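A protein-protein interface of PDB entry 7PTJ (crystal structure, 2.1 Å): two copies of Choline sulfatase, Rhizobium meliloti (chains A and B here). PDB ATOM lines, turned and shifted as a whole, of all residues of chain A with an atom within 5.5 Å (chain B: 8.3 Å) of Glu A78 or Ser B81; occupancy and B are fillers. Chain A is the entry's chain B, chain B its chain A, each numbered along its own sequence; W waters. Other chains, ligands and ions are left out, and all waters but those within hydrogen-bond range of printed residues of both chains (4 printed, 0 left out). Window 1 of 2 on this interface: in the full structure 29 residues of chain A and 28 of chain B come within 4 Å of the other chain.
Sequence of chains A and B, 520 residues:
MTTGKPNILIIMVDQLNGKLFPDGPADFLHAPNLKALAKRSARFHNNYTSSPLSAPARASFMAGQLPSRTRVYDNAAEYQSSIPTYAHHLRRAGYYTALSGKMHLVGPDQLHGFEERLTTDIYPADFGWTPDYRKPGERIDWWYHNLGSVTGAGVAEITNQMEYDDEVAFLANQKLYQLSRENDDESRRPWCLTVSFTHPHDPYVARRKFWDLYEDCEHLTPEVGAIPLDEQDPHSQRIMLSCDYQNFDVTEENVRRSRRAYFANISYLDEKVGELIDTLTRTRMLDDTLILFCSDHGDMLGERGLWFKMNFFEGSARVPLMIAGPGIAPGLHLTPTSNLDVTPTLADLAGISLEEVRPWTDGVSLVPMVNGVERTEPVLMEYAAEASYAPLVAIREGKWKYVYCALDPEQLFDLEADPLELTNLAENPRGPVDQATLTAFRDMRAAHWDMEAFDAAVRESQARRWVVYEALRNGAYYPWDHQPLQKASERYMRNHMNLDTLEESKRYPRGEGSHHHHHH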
ATOM      1  N   THR A  70     -11.762 -31.046  32.615  1.00  0.00           N
ATOM      2  CA  THR A  70     -12.954 -30.198  32.497  1.00  0.00           C
ATOM      3  C   THR A  70     -13.940 -30.733  31.464  1.00  0.00           C
ATOM      4  O   THR A  70     -15.135 -30.411  31.531  1.00  0.00           O
ATOM      5  CB  THR A  70     -12.594 -28.757  32.111  1.00  0.00           C
ATOM      6  OG1 THR A  70     -12.075 -28.726  30.770  1.00  0.00           O
ATOM      7  CG2 THR A  70     -11.574 -28.131  33.083  1.00  0.00           C
ATOM      8  N   ARG A  71     -13.470 -31.540  30.515  1.00  0.00           N
ATOM      9  CA  ARG A  71     -14.205 -32.004  29.340  1.00  0.00           C
ATOM     10  C   ARG A  71     -14.393 -30.911  28.290  1.00  0.00           C
ATOM     11  O   ARG A  71     -15.068 -31.155  27.281  1.00  0.00           O
ATOM     12  CB  ARG A  71     -15.593 -32.576  29.681  1.00  0.00           C
ATOM     13  CG  ARG A  71     -15.636 -33.462  30.911  1.00  0.00           C
ATOM     14  CD  ARG A  71     -14.641 -34.619  30.832  1.00  0.00           C
ATOM     15  NE  ARG A  71     -15.021 -35.671  31.765  1.00  0.00           N
ATOM     16  CZ  ARG A  71     -14.184 -36.284  32.593  1.00  0.00           C
ATOM     17  NH1 ARG A  71     -12.889 -36.014  32.593  1.00  0.00           N
ATOM     18  NH2 ARG A  71     -14.659 -37.185  33.445  1.00  0.00           N
ATOM     19  N   VAL A  72     -13.834 -29.721  28.476  1.00  0.00           N
ATOM     20  CA  VAL A  72     -14.006 -28.644  27.477  1.00  0.00           C
ATOM     21  C   VAL A  72     -12.885 -28.830  26.464  1.00  0.00           C
ATOM     22  O   VAL A  72     -11.808 -28.243  26.550  1.00  0.00           O
ATOM     23  CB  VAL A  72     -14.037 -27.249  28.105  1.00  0.00           C
ATOM     24  CG1 VAL A  72     -14.228 -26.168  27.015  1.00  0.00           C
ATOM     25  CG2 VAL A  72     -15.162 -27.160  29.144  1.00  0.00           C
ATOM     26  N   ALA A  76     -16.818 -25.498  21.427  1.00  0.00           N
ATOM     27  CA  ALA A  76     -18.261 -25.689  21.522  1.00  0.00           C
ATOM     28  C   ALA A  76     -18.656 -26.701  22.592  1.00  0.00           C
ATOM     29  O   ALA A  76     -19.812 -27.129  22.613  1.00  0.00           O
ATOM     30  CB  ALA A  76     -18.840 -26.124  20.167  1.00  0.00           C
ATOM     31  N   ALA A  77     -17.737 -27.084  23.483  1.00  0.00           N
ATOM     32  CA  ALA A  77     -18.010 -28.113  24.483  1.00  0.00           C
ATOM     33  C   ALA A  77     -18.563 -27.490  25.760  1.00  0.00           C
ATOM     34  O   ALA A  77     -17.994 -26.528  26.285  1.00  0.00           O
ATOM     35  CB  ALA A  77     -16.743 -28.908  24.803  1.00  0.00           C
ATOM     36  N   GLU A  78     -19.656 -28.061  26.268  1.00  0.00           N
ATOM     37  CA  GLU A  78     -20.287 -27.553  27.477  1.00  0.00           C
ATOM     38  C   GLU A  78     -19.337 -27.606  28.670  1.00  0.00           C
ATOM     39  O   GLU A  78     -18.641 -28.601  28.908  1.00  0.00           O
ATOM     40  CB  GLU A  78     -21.550 -28.350  27.795  1.00  0.00           C
ATOM     41  CG  GLU A  78     -22.235 -27.951  29.142  1.00  0.00           C
ATOM     42  CD  GLU A  78     -23.387 -28.862  29.468  1.00  0.00           C
ATOM     43  OE1 GLU A  78     -23.411 -29.997  28.936  1.00  0.00           O
ATOM     44  OE2 GLU A  78     -24.296 -28.448  30.223  1.00  0.00           O
ATOM     45  N   TYR A  79     -19.319 -26.518  29.417  1.00  0.00           N
ATOM     46  CA  TYR A  79     -18.589 -26.406  30.674  1.00  0.00           C
ATOM     47  C   TYR A  79     -19.599 -26.534  31.809  1.00  0.00           C
ATOM     48  O   TYR A  79     -20.471 -25.675  31.962  1.00  0.00           O
ATOM     49  CB  TYR A  79     -17.882 -25.061  30.701  1.00  0.00           C
ATOM     50  CG  TYR A  79     -16.828 -24.800  31.737  1.00  0.00           C
ATOM     51  CD1 TYR A  79     -16.210 -25.821  32.431  1.00  0.00           C
ATOM     52  CD2 TYR A  79     -16.432 -23.488  31.995  1.00  0.00           C
ATOM     53  CE1 TYR A  79     -15.217 -25.539  33.357  1.00  0.00           C
ATOM     54  CE2 TYR A  79     -15.452 -23.198  32.908  1.00  0.00           C
ATOM     55  CZ  TYR A  79     -14.842 -24.228  33.588  1.00  0.00           C
ATOM     56  OH  TYR A  79     -13.847 -23.934  34.496  1.00  0.00           O
ATOM     57  N   GLN A  80     -19.497 -27.610  32.583  1.00  0.00           N
ATOM     58  CA  GLN A  80     -20.469 -27.892  33.635  1.00  0.00           C
ATOM     59  C   GLN A  80     -20.395 -26.845  34.734  1.00  0.00           C
ATOM     60  O   GLN A  80     -19.311 -26.431  35.129  1.00  0.00           O
ATOM     61  CB  GLN A  80     -20.205 -29.277  34.229  1.00  0.00           C
ATOM     62  CG  GLN A  80     -20.437 -30.396  33.240  1.00  0.00           C
ATOM     63  CD  GLN A  80     -19.682 -31.659  33.621  1.00  0.00           C
ATOM     64  OE1 GLN A  80     -18.635 -31.989  33.030  1.00  0.00           O
ATOM     65  NE2 GLN A  80     -20.193 -32.364  34.626  1.00  0.00           N
ATOM     66  N   VAL A 106     -19.032 -21.997  27.282  1.00  0.00           N
ATOM     67  CA  VAL A 106     -20.039 -22.607  26.422  1.00  0.00           C
ATOM     68  C   VAL A 106     -21.066 -23.316  27.300  1.00  0.00           C
ATOM     69  O   VAL A 106     -20.710 -24.082  28.205  1.00  0.00           O
ATOM     70  CB  VAL A 106     -19.403 -23.561  25.396  1.00  0.00           C
ATOM     71  CG1 VAL A 106     -20.454 -24.125  24.477  1.00  0.00           C
ATOM     72  CG2 VAL A 106     -18.337 -22.816  24.569  1.00  0.00           C
ATOM     73  N   GLY A 107     -22.342 -23.062  27.027  1.00  0.00           N
ATOM     74  CA  GLY A 107     -23.408 -23.638  27.799  1.00  0.00           C
ATOM     75  C   GLY A 107     -24.181 -22.562  28.522  1.00  0.00           C
ATOM     76  O   GLY A 107     -23.824 -21.377  28.496  1.00  0.00           O
ATOM     77  N   PRO A 108     -25.273 -22.965  29.176  1.00  0.00           N
ATOM     78  CA  PRO A 108     -26.193 -21.980  29.774  1.00  0.00           C
ATOM     79  C   PRO A 108     -25.638 -21.256  30.985  1.00  0.00           C
ATOM     80  O   PRO A 108     -26.155 -20.175  31.296  1.00  0.00           O
ATOM     81  CB  PRO A 108     -27.427 -22.814  30.158  1.00  0.00           C
ATOM     82  CG  PRO A 108     -26.970 -24.246  30.141  1.00  0.00           C
ATOM     83  CD  PRO A 108     -25.723 -24.361  29.324  1.00  0.00           C
ATOM     84  N   PHE A 127     -23.335 -24.687  20.982  1.00  0.00           N
ATOM     85  CA  PHE A 127     -22.522 -25.803  20.508  1.00  0.00           C
ATOM     86  C   PHE A 127     -22.186 -25.709  19.017  1.00  0.00           C
ATOM     87  O   PHE A 127     -21.776 -26.720  18.428  1.00  0.00           O
ATOM     88  CB  PHE A 127     -23.217 -27.149  20.784  1.00  0.00           C
ATOM     89  CG  PHE A 127     -23.625 -27.362  22.223  1.00  0.00           C
ATOM     90  CD1 PHE A 127     -22.875 -26.846  23.261  1.00  0.00           C
ATOM     91  CD2 PHE A 127     -24.772 -28.091  22.528  1.00  0.00           C
ATOM     92  CE1 PHE A 127     -23.264 -27.051  24.592  1.00  0.00           C
ATOM     93  CE2 PHE A 127     -25.157 -28.299  23.838  1.00  0.00           C
ATOM     94  CZ  PHE A 127     -24.398 -27.779  24.875  1.00  0.00           C
ATOM     95  N   ARG A 465     -23.174 -33.519  20.947  1.00  0.00           N
ATOM     96  CA  ARG A 465     -23.526 -32.171  20.514  1.00  0.00           C
ATOM     97  C   ARG A 465     -24.088 -32.146  19.098  1.00  0.00           C
ATOM     98  O   ARG A 465     -24.932 -31.298  18.784  1.00  0.00           O
ATOM     99  CB  ARG A 465     -22.306 -31.267  20.628  1.00  0.00           C
ATOM    100  CG  ARG A 465     -21.969 -30.954  22.059  1.00  0.00           C
ATOM    101  CD  ARG A 465     -20.709 -30.115  22.122  1.00  0.00           C
ATOM    102  NE  ARG A 465     -19.505 -30.930  22.141  1.00  0.00           N
ATOM    103  CZ  ARG A 465     -18.322 -30.511  21.710  1.00  0.00           C
ATOM    104  NH1 ARG A 465     -18.179 -29.334  21.115  1.00  0.00           N
ATOM    105  NH2 ARG A 465     -17.252 -31.280  21.904  1.00  0.00           N
ATOM    106  N   VAL A 468     -27.763 -32.856  19.741  1.00  0.00           N
ATOM    107  CA  VAL A 468     -28.459 -31.807  20.484  1.00  0.00           C
ATOM    108  C   VAL A 468     -28.483 -30.498  19.702  1.00  0.00           C
ATOM    109  O   VAL A 468     -29.496 -29.793  19.680  1.00  0.00           O
ATOM    110  CB  VAL A 468     -27.797 -31.620  21.863  1.00  0.00           C
ATOM    111  CG1 VAL A 468     -28.265 -30.314  22.513  1.00  0.00           C
ATOM    112  CG2 VAL A 468     -28.134 -32.778  22.742  1.00  0.00           C
ATOM    113  N   TRP A 480     -28.353 -18.447  25.020  1.00  0.00           N
ATOM    114  CA  TRP A 480     -27.655 -18.577  26.291  1.00  0.00           C
ATOM    115  C   TRP A 480     -26.758 -17.378  26.581  1.00  0.00           C
ATOM    116  O   TRP A 480     -26.142 -17.313  27.648  1.00  0.00           O
ATOM    117  CB  TRP A 480     -26.836 -19.884  26.306  1.00  0.00           C
ATOM    118  CG  TRP A 480     -27.694 -21.131  26.398  1.00  0.00           C
ATOM    119  CD1 TRP A 480     -29.003 -21.209  26.833  1.00  0.00           C
ATOM    120  CD2 TRP A 480     -27.314 -22.473  26.045  1.00  0.00           C
ATOM    121  NE1 TRP A 480     -29.440 -22.502  26.769  1.00  0.00           N
ATOM    122  CE2 TRP A 480     -28.435 -23.299  26.286  1.00  0.00           C
ATOM    123  CE3 TRP A 480     -26.134 -23.053  25.543  1.00  0.00           C
ATOM    124  CZ2 TRP A 480     -28.415 -24.677  26.053  1.00  0.00           C
ATOM    125  CZ3 TRP A 480     -26.117 -24.420  25.307  1.00  0.00           C
ATOM    126  CH2 TRP A 480     -27.248 -25.218  25.564  1.00  0.00           C
ATOM    127  N   GLU B  78     -26.494 -31.696  38.894  1.00  0.00           N
ATOM    128  CA  GLU B  78     -26.627 -30.969  37.633  1.00  0.00           C
ATOM    129  C   GLU B  78     -26.909 -31.897  36.464  1.00  0.00           C
ATOM    130  O   GLU B  78     -26.228 -32.907  36.268  1.00  0.00           O
ATOM    131  CB  GLU B  78     -25.357 -30.169  37.348  1.00  0.00           C
ATOM    132  CG  GLU B  78     -25.334 -29.537  35.950  1.00  0.00           C
ATOM    133  CD  GLU B  78     -24.034 -28.799  35.645  1.00  0.00           C
ATOM    134  OE1 GLU B  78     -23.005 -29.086  36.294  1.00  0.00           O
ATOM    135  OE2 GLU B  78     -24.043 -27.916  34.758  1.00  0.00           O
ATOM    136  N   TYR B  79     -27.866 -31.512  35.636  1.00  0.00           N
ATOM    137  CA  TYR B  79     -28.208 -32.256  34.428  1.00  0.00           C
ATOM    138  C   TYR B  79     -27.565 -31.535  33.252  1.00  0.00           C
ATOM    139  O   TYR B  79     -27.957 -30.410  32.916  1.00  0.00           O
ATOM    140  CB  TYR B  79     -29.726 -32.335  34.281  1.00  0.00           C
ATOM    141  CG  TYR B  79     -30.319 -33.312  33.266  1.00  0.00           C
ATOM    142  CD1 TYR B  79     -29.581 -34.370  32.711  1.00  0.00           C
ATOM    143  CD2 TYR B  79     -31.661 -33.176  32.891  1.00  0.00           C
ATOM    144  CE1 TYR B  79     -30.183 -35.250  31.808  1.00  0.00           C
ATOM    145  CE2 TYR B  79     -32.257 -34.033  32.012  1.00  0.00           C
ATOM    146  CZ  TYR B  79     -31.524 -35.075  31.473  1.00  0.00           C
ATOM    147  OH  TYR B  79     -32.174 -35.918  30.616  1.00  0.00           O
ATOM    148  N   GLN B  80     -26.574 -32.178  32.634  1.00  0.00           N
ATOM    149  CA  GLN B  80     -25.820 -31.554  31.549  1.00  0.00           C
ATOM    150  C   GLN B  80     -26.713 -31.245  30.352  1.00  0.00           C
ATOM    151  O   GLN B  80     -27.510 -32.077  29.914  1.00  0.00           O
ATOM    152  CB  GLN B  80     -24.664 -32.468  31.113  1.00  0.00           C
ATOM    153  CG  GLN B  80     -23.605 -32.655  32.188  1.00  0.00           C
ATOM    154  CD  GLN B  80     -22.675 -33.824  31.903  1.00  0.00           C
ATOM    155  OE1 GLN B  80     -22.732 -34.865  32.578  1.00  0.00           O
ATOM    156  NE2 GLN B  80     -21.817 -33.664  30.897  1.00  0.00           N
ATOM    157  N   SER B  81     -26.555 -30.044  29.797  1.00  0.00           N
ATOM    158  CA  SER B  81     -27.428 -29.669  28.706  1.00  0.00           C
ATOM    159  C   SER B  81     -27.065 -30.364  27.396  1.00  0.00           C
ATOM    160  O   SER B  81     -27.869 -30.341  26.456  1.00  0.00           O
ATOM    161  CB  SER B  81     -27.441 -28.132  28.568  1.00  0.00           C
ATOM    162  OG  SER B  81     -26.359 -27.669  27.788  1.00  0.00           O
ATOM    163  N   SER B  82     -25.923 -31.034  27.321  1.00  0.00           N
ATOM    164  CA  SER B  82     -25.575 -31.782  26.124  1.00  0.00           C
ATOM    165  C   SER B  82     -26.163 -33.194  26.091  1.00  0.00           C
ATOM    166  O   SER B  82     -25.917 -33.921  25.130  1.00  0.00           O
ATOM    167  CB  SER B  82     -24.042 -31.850  25.978  1.00  0.00           C
ATOM    168  OG  SER B  82     -23.485 -32.612  27.030  1.00  0.00           O
ATOM    169  N   ILE B  83     -26.920 -33.615  27.100  1.00  0.00           N
ATOM    170  CA  ILE B  83     -27.485 -34.969  27.084  1.00  0.00           C
ATOM    171  C   ILE B  83     -28.758 -35.003  26.239  1.00  0.00           C
ATOM    172  O   ILE B  83     -29.697 -34.252  26.514  1.00  0.00           O
ATOM    173  CB  ILE B  83     -27.772 -35.470  28.505  1.00  0.00           C
ATOM    174  CG1 ILE B  83     -26.459 -35.641  29.281  1.00  0.00           C
ATOM    175  CG2 ILE B  83     -28.499 -36.798  28.428  1.00  0.00           C
ATOM    176  CD1 ILE B  83     -26.669 -35.973  30.751  1.00  0.00           C
ATOM    177  N   PRO B  84     -28.843 -35.847  25.212  1.00  0.00           N
ATOM    178  CA  PRO B  84     -30.050 -35.877  24.370  1.00  0.00           C
ATOM    179  C   PRO B  84     -31.255 -36.379  25.148  1.00  0.00           C
ATOM    180  O   PRO B  84     -31.170 -37.389  25.847  1.00  0.00           O
ATOM    181  CB  PRO B  84     -29.684 -36.851  23.244  1.00  0.00           C
ATOM    182  CG  PRO B  84     -28.211 -36.990  23.303  1.00  0.00           C
ATOM    183  CD  PRO B  84     -27.827 -36.794  24.747  1.00  0.00           C
ATOM    184  N   THR B  85     -32.383 -35.681  25.004  1.00  0.00           N
ATOM    185  CA  THR B  85     -33.650 -36.108  25.577  1.00  0.00           C
ATOM    186  C   THR B  85     -34.656 -36.389  24.466  1.00  0.00           C
ATOM    187  O   THR B  85     -34.405 -36.126  23.288  1.00  0.00           O
ATOM    188  CB  THR B  85     -34.229 -35.051  26.517  1.00  0.00           C
ATOM    189  OG1 THR B  85     -34.736 -33.955  25.739  1.00  0.00           O
ATOM    190  CG2 THR B  85     -33.178 -34.587  27.539  1.00  0.00           C
ATOM    191  N   HIS B  88     -35.145 -33.398  22.343  1.00  0.00           N
ATOM    192  CA  HIS B  88     -34.181 -33.270  21.250  1.00  0.00           C
ATOM    193  C   HIS B  88     -34.532 -34.211  20.109  1.00  0.00           C
ATOM    194  O   HIS B  88     -34.562 -33.804  18.934  1.00  0.00           O
ATOM    195  CB  HIS B  88     -32.754 -33.553  21.729  1.00  0.00           C
ATOM    196  CG  HIS B  88     -32.237 -32.574  22.735  1.00  0.00           C
ATOM    197  ND1 HIS B  88     -32.077 -32.900  24.063  1.00  0.00           N
ATOM    198  CD2 HIS B  88     -31.812 -31.292  22.607  1.00  0.00           C
ATOM    199  CE1 HIS B  88     -31.602 -31.853  24.718  1.00  0.00           C
ATOM    200  NE2 HIS B  88     -31.418 -30.869  23.857  1.00  0.00           N
ATOM    201  N   VAL B 106     -32.142 -29.727  37.346  1.00  0.00           N
ATOM    202  CA  VAL B 106     -31.233 -28.955  38.186  1.00  0.00           C
ATOM    203  C   VAL B 106     -30.087 -28.448  37.331  1.00  0.00           C
ATOM    204  O   VAL B 106     -29.460 -29.219  36.589  1.00  0.00           O
ATOM    205  CB  VAL B 106     -30.712 -29.779  39.374  1.00  0.00           C
ATOM    206  CG1 VAL B 106     -29.773 -28.923  40.250  1.00  0.00           C
ATOM    207  CG2 VAL B 106     -31.872 -30.260  40.199  1.00  0.00           C
ATOM    208  N   GLY B 107     -29.783 -27.164  37.468  1.00  0.00           N
ATOM    209  CA  GLY B 107     -28.760 -26.553  36.655  1.00  0.00           C
ATOM    210  C   GLY B 107     -29.362 -25.434  35.831  1.00  0.00           C
ATOM    211  O   GLY B 107     -30.579 -25.235  35.819  1.00  0.00           O
ATOM    212  N   PRO B 108     -28.516 -24.660  35.147  1.00  0.00           N
ATOM    213  CA  PRO B 108     -29.021 -23.473  34.452  1.00  0.00           C
ATOM    214  C   PRO B 108     -29.806 -23.790  33.196  1.00  0.00           C
ATOM    215  O   PRO B 108     -30.495 -22.899  32.697  1.00  0.00           O
ATOM    216  CB  PRO B 108     -27.744 -22.682  34.128  1.00  0.00           C
ATOM    217  CG  PRO B 108     -26.711 -23.705  34.009  1.00  0.00           C
ATOM    218  CD  PRO B 108     -27.053 -24.765  35.058  1.00  0.00           C
ATOM    219  N   ASP B 109     -29.707 -25.004  32.646  1.00  0.00           N
ATOM    220  CA  ASP B 109     -30.567 -25.395  31.526  1.00  0.00           C
ATOM    221  C   ASP B 109     -31.903 -25.861  32.087  1.00  0.00           C
ATOM    222  O   ASP B 109     -31.982 -26.922  32.708  1.00  0.00           O
ATOM    223  CB  ASP B 109     -29.932 -26.502  30.682  1.00  0.00           C
ATOM    224  CG  ASP B 109     -30.723 -26.785  29.384  1.00  0.00           C
ATOM    225  OD1 ASP B 109     -31.765 -26.143  29.152  1.00  0.00           O
ATOM    226  OD2 ASP B 109     -30.305 -27.632  28.585  1.00  0.00           O
ATOM    227  N   GLN B 110     -32.952 -25.072  31.878  1.00  0.00           N
ATOM    228  CA  GLN B 110     -34.287 -25.424  32.340  1.00  0.00           C
ATOM    229  C   GLN B 110     -35.198 -25.896  31.208  1.00  0.00           C
ATOM    230  O   GLN B 110     -36.416 -26.024  31.413  1.00  0.00           O
ATOM    231  CB  GLN B 110     -34.925 -24.232  33.070  1.00  0.00           C
ATOM    232  CG  GLN B 110     -34.306 -23.966  34.429  1.00  0.00           C
ATOM    233  CD  GLN B 110     -34.510 -25.130  35.374  1.00  0.00           C
ATOM    234  OE1 GLN B 110     -35.638 -25.468  35.705  1.00  0.00           O
ATOM    235  NE2 GLN B 110     -33.413 -25.741  35.826  1.00  0.00           N
ATOM    236  N   LEU B 111     -34.634 -26.159  30.025  1.00  0.00           N
ATOM    237  CA  LEU B 111     -35.368 -26.632  28.858  1.00  0.00           C
ATOM    238  C   LEU B 111     -34.945 -28.015  28.392  1.00  0.00           C
ATOM    239  O   LEU B 111     -35.797 -28.822  28.037  1.00  0.00           O
ATOM    240  CB  LEU B 111     -35.184 -25.640  27.694  1.00  0.00           C
ATOM    241  CG  LEU B 111     -35.739 -24.238  27.932  1.00  0.00           C
ATOM    242  CD1 LEU B 111     -35.452 -23.308  26.734  1.00  0.00           C
ATOM    243  CD2 LEU B 111     -37.234 -24.336  28.198  1.00  0.00           C
ATOM    244  N   HIS B 112     -33.640 -28.286  28.340  1.00  0.00           N
ATOM    245  CA  HIS B 112     -33.120 -29.584  27.939  1.00  0.00           C
ATOM    246  C   HIS B 112     -33.804 -30.094  26.674  1.00  0.00           C
ATOM    247  O   HIS B 112     -34.317 -31.215  26.619  1.00  0.00           O
ATOM    248  CB  HIS B 112     -33.244 -30.579  29.080  1.00  0.00           C
ATOM    249  CG  HIS B 112     -32.186 -30.396  30.117  1.00  0.00           C
ATOM    250  ND1 HIS B 112     -30.940 -30.986  30.015  1.00  0.00           N
ATOM    251  CD2 HIS B 112     -32.166 -29.659  31.252  1.00  0.00           C
ATOM    252  CE1 HIS B 112     -30.206 -30.629  31.054  1.00  0.00           C
ATOM    253  NE2 HIS B 112     -30.928 -29.835  31.825  1.00  0.00           N
ATOM    254  N   GLY B 113     -33.795 -29.258  25.629  1.00  0.00           N
ATOM    255  CA  GLY B 113     -34.386 -29.628  24.352  1.00  0.00           C
ATOM    256  C   GLY B 113     -35.791 -29.095  24.115  1.00  0.00           C
ATOM    257  O   GLY B 113     -36.154 -28.846  22.956  1.00  0.00           O
HETATM  258  O   HOH W   1     -21.605 -31.880  29.142  1.00  0.00           O
HETATM  259  O   HOH W   2     -24.798 -27.019  32.294  1.00  0.00           O
HETATM  260  O   HOH W   3     -31.896 -23.916  27.688  1.00  0.00           O
HETATM  261  O   HOH W   4     -22.073 -31.742  36.344  1.00  0.00           O
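Printed residues of chain A that touch a printed residue of chain B: Glu A78, Gln A80, Pro A108, Phe A127, Val A468 and Trp A480. Hydrophobic or aromatic side chains of chain A within 4 Å of the printed part of chain B: Pro A108, Phe A127, Val A468 and Trp A480. Of the 17 printed residues of chain B, 8 touch a printed residue of chain A. Among the printed residues, no Asp or Glu carboxylate lies within 4 Å of a Lys or Arg side-chain nitrogen of the other chain.
OE1 of Glu A78 lies within hydrogen-bond range of N of Ser B82, at 3.2 Å. The side-chain carboxylate of Glu A78 sits at hydrogen-bond distance from the backbone NH of Ser B81 (2.8 Å).
N of His B112 lies within hydrogen-bond range of OD1 of Asp B109 (3.0 Å). The backbone NH (N) of Thr B85 sits at hydrogen-bond distance from a ring nitrogen (ND1) of His B88 (3.0 Å). A ring nitrogen (NE2) of His B88 sits close to the backbone NH (N) of Gly B113 (3.4 Å). The side-chain carboxylate (OD1) of Asp B109 is in hydrogen-bond range of the backbone NH (N) of Leu B111 (3.0 Å).
Water W1 lies within hydrogen-bond range of the side-chain amide nitrogen (NE2) of Gln B80 (2.5 Å), the side-chain carboxylate (OE1) of Glu A78 (2.6 Å) and the side-chain hydroxyl (OG) of Ser B82 (2.9 Å). Water W2 lies within hydrogen-bond range of OE2 of Glu A78 (2.6 Å) and OE2 of Glu B78 (2.7 Å). Water W4 bridges the side-chain amide nitrogen (NE2) of Gln A80 (2.6 Å) and the side-chain carboxylate (OE1) of Glu B78 (2.8 Å). Water W3 bridges the side-chain carboxylate (OD1) of Asp B109 (2.7 Å) and the indole nitrogen (NE1) of Trp A480 (3.0 Å).
Of the printed residues of chain B, Glu A78 touches Gln B80, Ser B81 and Ser B82. Ser B81 touches just these residues of chain A: Glu A78 (2.8 Å), Pro A108 (3.7 Å), Phe A127 (3.5 Å), Val A468 (3.96 Å) and Trp A480 (3.4 Å). No residue of chain B comes within 4 Å of Ala A77. Of the printed residues of chain A, His B88 touches Val A468. Printed residues of chain A within 4 Å of Ser B82: Glu A78 and Val A468. Of the printed residues of chain B, Trp A480 touches Ser B81 (3.4 Å). Ala A76 touches none of the printed residues of chain B. The nearest residue of chain A that does not touch Ser B81 is Gly A107 (5.0 Å).
Among the printed residues, pairs that only touch across the chains: Glu A78 with Gln B80 (3.5 Å), Gln A80 with Glu B78 (3.5 Å), Gln A80 with Gln B80 (3.96 Å), Pro A108 with Ser B81 (3.7 Å), Pro A108 with Pro B108 (3.9 Å), Pro A108 with Asp B109 (3.8 Å), Phe A127 with Ser B81 (3.5 Å), Val A468 with Ser B81 (3.96 Å), Val A468 with Ser B82 (3.5 Å), Val A468 with Pro B84 (3.99 Å), Val A468 with His B88 (3.5 Å) and Trp A480 with Ser B81 (3.4 Å).
Glu A78 touches Gln B80, and with the chains exchanged Gln A80 touches Glu B78. Gln A80 touches its own counterpart, Gln B80. Pro A108 touches its own counterpart, Pro B108.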
